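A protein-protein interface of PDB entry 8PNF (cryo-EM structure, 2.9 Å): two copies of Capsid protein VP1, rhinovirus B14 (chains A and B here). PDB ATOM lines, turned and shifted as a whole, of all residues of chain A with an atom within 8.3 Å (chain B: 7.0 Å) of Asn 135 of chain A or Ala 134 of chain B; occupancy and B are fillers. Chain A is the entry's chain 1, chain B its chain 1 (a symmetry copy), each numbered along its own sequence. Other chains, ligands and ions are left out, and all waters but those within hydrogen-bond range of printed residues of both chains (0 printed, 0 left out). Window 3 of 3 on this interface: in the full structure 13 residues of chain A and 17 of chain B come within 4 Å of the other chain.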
ATOM      1  N   GLN A 130      10.682  16.632 -15.300  1.00  0.00           N
ATOM      2  CA  GLN A 130      10.334  15.749 -16.407  1.00  0.00           C
ATOM      3  C   GLN A 130       9.670  16.578 -17.492  1.00  0.00           C
ATOM      4  O   GLN A 130       8.449  16.793 -17.447  1.00  0.00           O
ATOM      5  CB  GLN A 130       9.412  14.608 -15.965  1.00  0.00           C
ATOM      6  CG  GLN A 130      10.021  13.583 -15.016  1.00  0.00           C
ATOM      7  CD  GLN A 130      10.012  14.025 -13.573  1.00  0.00           C
ATOM      8  OE1 GLN A 130       9.287  14.945 -13.198  1.00  0.00           O
ATOM      9  NE2 GLN A 130      10.811  13.363 -12.750  1.00  0.00           N
ATOM     10  N   ASP A 132       9.237  15.728 -20.641  1.00  0.00           N
ATOM     11  CA  ASP A 132       8.433  14.860 -21.484  1.00  0.00           C
ATOM     12  C   ASP A 132       7.346  14.205 -20.633  1.00  0.00           C
ATOM     13  O   ASP A 132       7.301  14.376 -19.413  1.00  0.00           O
ATOM     14  CB  ASP A 132       9.320  13.834 -22.185  1.00  0.00           C
ATOM     15  CG  ASP A 132      10.447  14.479 -22.968  1.00  0.00           C
ATOM     16  OD1 ASP A 132      10.276  15.626 -23.428  1.00  0.00           O
ATOM     17  OD2 ASP A 132      11.506  13.836 -23.127  1.00  0.00           O
ATOM     18  N   SER A 133       6.454  13.458 -21.281  1.00  0.00           N
ATOM     19  CA  SER A 133       5.315  12.859 -20.598  1.00  0.00           C
ATOM     20  C   SER A 133       5.766  11.756 -19.652  1.00  0.00           C
ATOM     21  O   SER A 133       6.533  10.869 -20.034  1.00  0.00           O
ATOM     22  CB  SER A 133       4.326  12.298 -21.615  1.00  0.00           C
ATOM     23  OG  SER A 133       3.426  11.395 -20.998  1.00  0.00           O
ATOM     24  N   ALA A 134       5.282  11.817 -18.415  1.00  0.00           N
ATOM     25  CA  ALA A 134       5.674  10.877 -17.380  1.00  0.00           C
ATOM     26  C   ALA A 134       4.475  10.596 -16.492  1.00  0.00           C
ATOM     27  O   ALA A 134       3.589  11.439 -16.335  1.00  0.00           O
ATOM     28  CB  ALA A 134       6.838  11.420 -16.547  1.00  0.00           C
ATOM     29  N   ASN A 135       4.454   9.400 -15.912  1.00  0.00           N
ATOM     30  CA  ASN A 135       3.358   8.995 -15.046  1.00  0.00           C
ATOM     31  C   ASN A 135       3.596   9.338 -13.588  1.00  0.00           C
ATOM     32  O   ASN A 135       2.632   9.398 -12.817  1.00  0.00           O
ATOM     33  CB  ASN A 135       3.118   7.489 -15.172  1.00  0.00           C
ATOM     34  CG  ASN A 135       2.522   7.111 -16.502  1.00  0.00           C
ATOM     35  OD1 ASN A 135       2.216   7.973 -17.323  1.00  0.00           O
ATOM     36  ND2 ASN A 135       2.362   5.817 -16.731  1.00  0.00           N
ATOM     37  N   TYR A 136       4.843   9.575 -13.202  1.00  0.00           N
ATOM     38  CA  TYR A 136       5.197   9.810 -11.812  1.00  0.00           C
ATOM     39  C   TYR A 136       6.498  10.594 -11.779  1.00  0.00           C
ATOM     40  O   TYR A 136       7.156  10.788 -12.803  1.00  0.00           O
ATOM     41  CB  TYR A 136       5.315   8.493 -11.031  1.00  0.00           C
ATOM     42  CG  TYR A 136       6.226   7.451 -11.654  1.00  0.00           C
ATOM     43  CD1 TYR A 136       5.735   6.523 -12.564  1.00  0.00           C
ATOM     44  CD2 TYR A 136       7.570   7.382 -11.311  1.00  0.00           C
ATOM     45  CE1 TYR A 136       6.561   5.576 -13.130  1.00  0.00           C
ATOM     46  CE2 TYR A 136       8.401   6.438 -11.870  1.00  0.00           C
ATOM     47  CZ  TYR A 136       7.892   5.537 -12.779  1.00  0.00           C
ATOM     48  OH  TYR A 136       8.720   4.592 -13.338  1.00  0.00           O
ATOM     49  N   SER A 137       6.854  11.057 -10.587  1.00  0.00           N
ATOM     50  CA  SER A 137       8.127  11.718 -10.345  1.00  0.00           C
ATOM     51  C   SER A 137       9.067  10.710  -9.701  1.00  0.00           C
ATOM     52  O   SER A 137       8.728  10.112  -8.676  1.00  0.00           O
ATOM     53  CB  SER A 137       7.946  12.940  -9.447  1.00  0.00           C
ATOM     54  OG  SER A 137       9.173  13.618  -9.255  1.00  0.00           O
ATOM     55  N   SER A 138      10.238  10.524 -10.301  1.00  0.00           N
ATOM     56  CA  SER A 138      11.163   9.503  -9.833  1.00  0.00           C
ATOM     57  C   SER A 138      11.810   9.910  -8.515  1.00  0.00           C
ATOM     58  O   SER A 138      12.067  11.090  -8.268  1.00  0.00           O
ATOM     59  CB  SER A 138      12.238   9.242 -10.884  1.00  0.00           C
ATOM     60  OG  SER A 138      11.669   8.750 -12.081  1.00  0.00           O
ATOM     61  N   ASP A 227      13.997   4.704 -15.818  1.00  0.00           N
ATOM     62  CA  ASP A 227      12.567   4.464 -15.784  1.00  0.00           C
ATOM     63  C   ASP A 227      12.037   4.444 -17.212  1.00  0.00           C
ATOM     64  O   ASP A 227      12.799   4.432 -18.183  1.00  0.00           O
ATOM     65  CB  ASP A 227      11.873   5.524 -14.929  1.00  0.00           C
ATOM     66  CG  ASP A 227      11.943   5.212 -13.449  1.00  0.00           C
ATOM     67  OD1 ASP A 227      12.335   4.083 -13.098  1.00  0.00           O
ATOM     68  OD2 ASP A 227      11.613   6.097 -12.636  1.00  0.00           O
ATOM     69  N   GLU A 228      10.712   4.419 -17.348  1.00  0.00           N
ATOM     70  CA  GLU A 228      10.092   4.521 -18.662  1.00  0.00           C
ATOM     71  C   GLU A 228      10.269   5.901 -19.273  1.00  0.00           C
ATOM     72  O   GLU A 228      10.288   6.026 -20.502  1.00  0.00           O
ATOM     73  CB  GLU A 228       8.606   4.178 -18.565  1.00  0.00           C
ATOM     74  CG  GLU A 228       7.953   3.809 -19.885  1.00  0.00           C
ATOM     75  CD  GLU A 228       6.478   3.515 -19.733  1.00  0.00           C
ATOM     76  OE1 GLU A 228       5.840   3.123 -20.731  1.00  0.00           O
ATOM     77  OE2 GLU A 228       5.958   3.669 -18.610  1.00  0.00           O
ATOM     78  N   HIS A 229      10.413   6.931 -18.452  1.00  0.00           N
ATOM     79  CA  HIS A 229      10.532   8.300 -18.918  1.00  0.00           C
ATOM     80  C   HIS A 229      11.961   8.801 -18.743  1.00  0.00           C
ATOM     81  O   HIS A 229      12.845   8.096 -18.251  1.00  0.00           O
ATOM     82  CB  HIS A 229       9.541   9.204 -18.180  1.00  0.00           C
ATOM     83  CG  HIS A 229       9.618   9.102 -16.688  1.00  0.00           C
ATOM     84  ND1 HIS A 229       8.603   8.567 -15.927  1.00  0.00           N
ATOM     85  CD2 HIS A 229      10.578   9.488 -15.815  1.00  0.00           C
ATOM     86  CE1 HIS A 229       8.938   8.618 -14.651  1.00  0.00           C
ATOM     87  NE2 HIS A 229      10.132   9.171 -14.557  1.00  0.00           N
ATOM     88  N   GLN B 130      11.439   1.179 -11.981  1.00  0.00           N
ATOM     89  CA  GLN B 130      10.395   0.472 -12.713  1.00  0.00           C
ATOM     90  C   GLN B 130      10.689   0.586 -14.198  1.00  0.00           C
ATOM     91  O   GLN B 130      10.289   1.573 -14.834  1.00  0.00           O
ATOM     92  CB  GLN B 130       9.000   1.020 -12.399  1.00  0.00           C
ATOM     93  CG  GLN B 130       8.495   0.799 -10.979  1.00  0.00           C
ATOM     94  CD  GLN B 130       9.016   1.817  -9.994  1.00  0.00           C
ATOM     95  OE1 GLN B 130       9.501   2.880 -10.380  1.00  0.00           O
ATOM     96  NE2 GLN B 130       8.907   1.505  -8.712  1.00  0.00           N
ATOM     97  N   PRO B 131      11.388  -0.381 -14.798  1.00  0.00           N
ATOM     98  CA  PRO B 131      11.656  -0.303 -16.239  1.00  0.00           C
ATOM     99  C   PRO B 131      10.436  -0.553 -17.105  1.00  0.00           C
ATOM    100  O   PRO B 131      10.405  -0.079 -18.249  1.00  0.00           O
ATOM    101  CB  PRO B 131      12.719  -1.384 -16.457  1.00  0.00           C
ATOM    102  CG  PRO B 131      12.503  -2.351 -15.357  1.00  0.00           C
ATOM    103  CD  PRO B 131      11.959  -1.592 -14.185  1.00  0.00           C
ATOM    104  N   ASP B 132       9.435  -1.269 -16.608  1.00  0.00           N
ATOM    105  CA  ASP B 132       8.209  -1.483 -17.358  1.00  0.00           C
ATOM    106  C   ASP B 132       7.195  -0.405 -16.975  1.00  0.00           C
ATOM    107  O   ASP B 132       7.441   0.415 -16.086  1.00  0.00           O
ATOM    108  CB  ASP B 132       7.678  -2.893 -17.114  1.00  0.00           C
ATOM    109  CG  ASP B 132       8.709  -3.963 -17.421  1.00  0.00           C
ATOM    110  OD1 ASP B 132       9.578  -3.725 -18.283  1.00  0.00           O
ATOM    111  OD2 ASP B 132       8.647  -5.044 -16.799  1.00  0.00           O
ATOM    112  N   SER B 133       6.050  -0.396 -17.656  1.00  0.00           N
ATOM    113  CA  SER B 133       5.045   0.637 -17.450  1.00  0.00           C
ATOM    114  C   SER B 133       4.396   0.503 -16.082  1.00  0.00           C
ATOM    115  O   SER B 133       3.959  -0.584 -15.692  1.00  0.00           O
ATOM    116  CB  SER B 133       3.978   0.559 -18.540  1.00  0.00           C
ATOM    117  OG  SER B 133       2.818   1.276 -18.162  1.00  0.00           O
ATOM    118  N   ALA B 134       4.334   1.614 -15.354  1.00  0.00           N
ATOM    119  CA  ALA B 134       3.808   1.629 -14.001  1.00  0.00           C
ATOM    120  C   ALA B 134       3.069   2.938 -13.777  1.00  0.00           C
ATOM    121  O   ALA B 134       3.388   3.960 -14.388  1.00  0.00           O
ATOM    122  CB  ALA B 134       4.924   1.466 -12.968  1.00  0.00           C
ATOM    123  N   ASN B 135       2.075   2.895 -12.896  1.00  0.00           N
ATOM    124  CA  ASN B 135       1.277   4.073 -12.595  1.00  0.00           C
ATOM    125  C   ASN B 135       1.832   4.888 -11.442  1.00  0.00           C
ATOM    126  O   ASN B 135       1.492   6.069 -11.320  1.00  0.00           O
ATOM    127  CB  ASN B 135      -0.162   3.664 -12.270  1.00  0.00           C
ATOM    128  CG  ASN B 135      -0.908   3.173 -13.482  1.00  0.00           C
ATOM    129  OD1 ASN B 135      -0.386   3.196 -14.595  1.00  0.00           O
ATOM    130  ND2 ASN B 135      -2.133   2.715 -13.276  1.00  0.00           N
ATOM    131  N   TYR B 136       2.679   4.292 -10.613  1.00  0.00           N
ATOM    132  CA  TYR B 136       3.190   4.945  -9.419  1.00  0.00           C
ATOM    133  C   TYR B 136       4.505   4.285  -9.042  1.00  0.00           C
ATOM    134  O   TYR B 136       4.893   3.260  -9.606  1.00  0.00           O
ATOM    135  CB  TYR B 136       2.178   4.881  -8.266  1.00  0.00           C
ATOM    136  CG  TYR B 136       1.653   3.494  -7.943  1.00  0.00           C
ATOM    137  CD1 TYR B 136       0.520   2.993  -8.572  1.00  0.00           C
ATOM    138  CD2 TYR B 136       2.277   2.699  -6.990  1.00  0.00           C
ATOM    139  CE1 TYR B 136       0.041   1.734  -8.278  1.00  0.00           C
ATOM    140  CE2 TYR B 136       1.804   1.442  -6.690  1.00  0.00           C
ATOM    141  CZ  TYR B 136       0.686   0.964  -7.337  1.00  0.00           C
ATOM    142  OH  TYR B 136       0.211  -0.292  -7.038  1.00  0.00           O
ATOM    143  N   SER B 137       5.196   4.895  -8.086  1.00  0.00           N
ATOM    144  CA  SER B 137       6.411   4.338  -7.512  1.00  0.00           C
ATOM    145  C   SER B 137       6.052   3.698  -6.179  1.00  0.00           C
ATOM    146  O   SER B 137       5.466   4.355  -5.313  1.00  0.00           O
ATOM    147  CB  SER B 137       7.473   5.419  -7.326  1.00  0.00           C
ATOM    148  OG  SER B 137       8.675   4.872  -6.819  1.00  0.00           O
ATOM    149  N   HIS B 229       2.568  -3.789 -11.126  1.00  0.00           N
ATOM    150  CA  HIS B 229       3.770  -3.691 -11.931  1.00  0.00           C
ATOM    151  C   HIS B 229       4.914  -4.456 -11.277  1.00  0.00           C
ATOM    152  O   HIS B 229       4.778  -5.043 -10.201  1.00  0.00           O
ATOM    153  CB  HIS B 229       4.148  -2.223 -12.153  1.00  0.00           C
ATOM    154  CG  HIS B 229       4.241  -1.422 -10.891  1.00  0.00           C
ATOM    155  ND1 HIS B 229       3.358  -0.411 -10.588  1.00  0.00           N
ATOM    156  CD2 HIS B 229       5.127  -1.468  -9.868  1.00  0.00           C
ATOM    157  CE1 HIS B 229       3.690   0.125  -9.428  1.00  0.00           C
ATOM    158  NE2 HIS B 229       4.758  -0.499  -8.971  1.00  0.00           N
ATOM    159  N   LYS B 230       6.059  -4.429 -11.947  1.00  0.00           N
ATOM    160  CA  LYS B 230       7.295  -5.031 -11.472  1.00  0.00           C
ATOM    161  C   LYS B 230       8.289  -3.917 -11.178  1.00  0.00           C
ATOM    162  O   LYS B 230       8.510  -3.042 -12.022  1.00  0.00           O
ATOM    163  CB  LYS B 230       7.850  -5.993 -12.525  1.00  0.00           C
ATOM    164  CG  LYS B 230       9.269  -6.476 -12.296  1.00  0.00           C
ATOM    165  CD  LYS B 230       9.585  -7.628 -13.244  1.00  0.00           C
ATOM    166  CE  LYS B 230      10.795  -8.428 -12.785  1.00  0.00           C
ATOM    167  NZ  LYS B 230      11.715  -8.772 -13.908  1.00  0.00           N
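Of the 11 printed residues of chain A, 4 touch a printed residue of chain B.
Among the printed residues, no Asp or Glu carboxylate lies within 4 Å of a Lys or Arg side-chain nitrogen of the other chain.
The side-chain hydroxyl of Tyr 136 of chain A sits close to the side-chain carboxylate of Asp 227 of chain A (3.3 Å).
OG of Ser 138 of chain A sits at hydrogen-bond distance from OD2 of Asp 227 of chain A (2.7 Å).
The side-chain amide nitrogen (ND2) of Asn 135 of chain A is in hydrogen-bond range of the backbone carbonyl oxygen (O) of Ala 134 of chain B (3.2 Å).
The side-chain carboxylate of Asp 227 of chain A lies within hydrogen-bond range of the backbone NH of Gln 130 of chain B (3.2 Å).
Asn 135 of chain A touches Ala 134 of chain B, but with the chains exchanged Ala 134 of chain A does not touch Asn 135 of chain B (7.5 Å).
Asn 135 of chain B touches its own counterpart, Asn 135 of chain A.
Tyr 136 of chain A touches Gln 130 of chain B, but with the chains exchanged Gln 130 of chain A does not touch Tyr 136 of chain B (11.7 Å).
Tyr 136 of chain A touches Ala 134 of chain B, but with the chains exchanged Ala 134 of chain A does not touch Tyr 136 of chain B (8.8 Å).
8 positions are printed for both chains.
Of the 7 pairs that touch across the chains among the printed residues, 1 has its exchanged pair printed and touching as well.
Among the printed residues, pairs that only touch across the chains: Glu 228 of chain A with Ser 133 of chain B (3.4 Å), Tyr 136 of chain A with Gln 130 of chain B (3.5 Å), Tyr 136 of chain A with Ala 134 of chain B (3.8 Å), Glu 228 of chain A with Gln 130 of chain B (3.8 Å) and Asn 135 of chain A with Asn 135 of chain B (3.8 Å).
Asn 135 of chain A touches just these residues of chain B: Ala 134 and Asn 135.
Of chain A, only Asn 135 and Tyr 136 come within 4 Å of Ala 134 of chain B.
Of the printed residues of chain A, Asn 135 of chain B touches Asn 135.
Of the printed residues of chain A, Gln 130 of chain B touches Tyr 136, Asp 227 and Glu 228.
Printed residues of chain B within 4 Å of Glu 228 of chain A: Gln 130 (3.8 Å) and Ser 133 (3.4 Å).
Pro 131 of chain B touches none of the printed residues of chain A.
The nearest residue of chain A that does not touch Ala 134 of chain B is Glu 228 of chain A (4.2 Å).
The nearest printed residue of chain B that does not touch Tyr 136 of chain A is Tyr 136 of chain B (4.3 Å).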
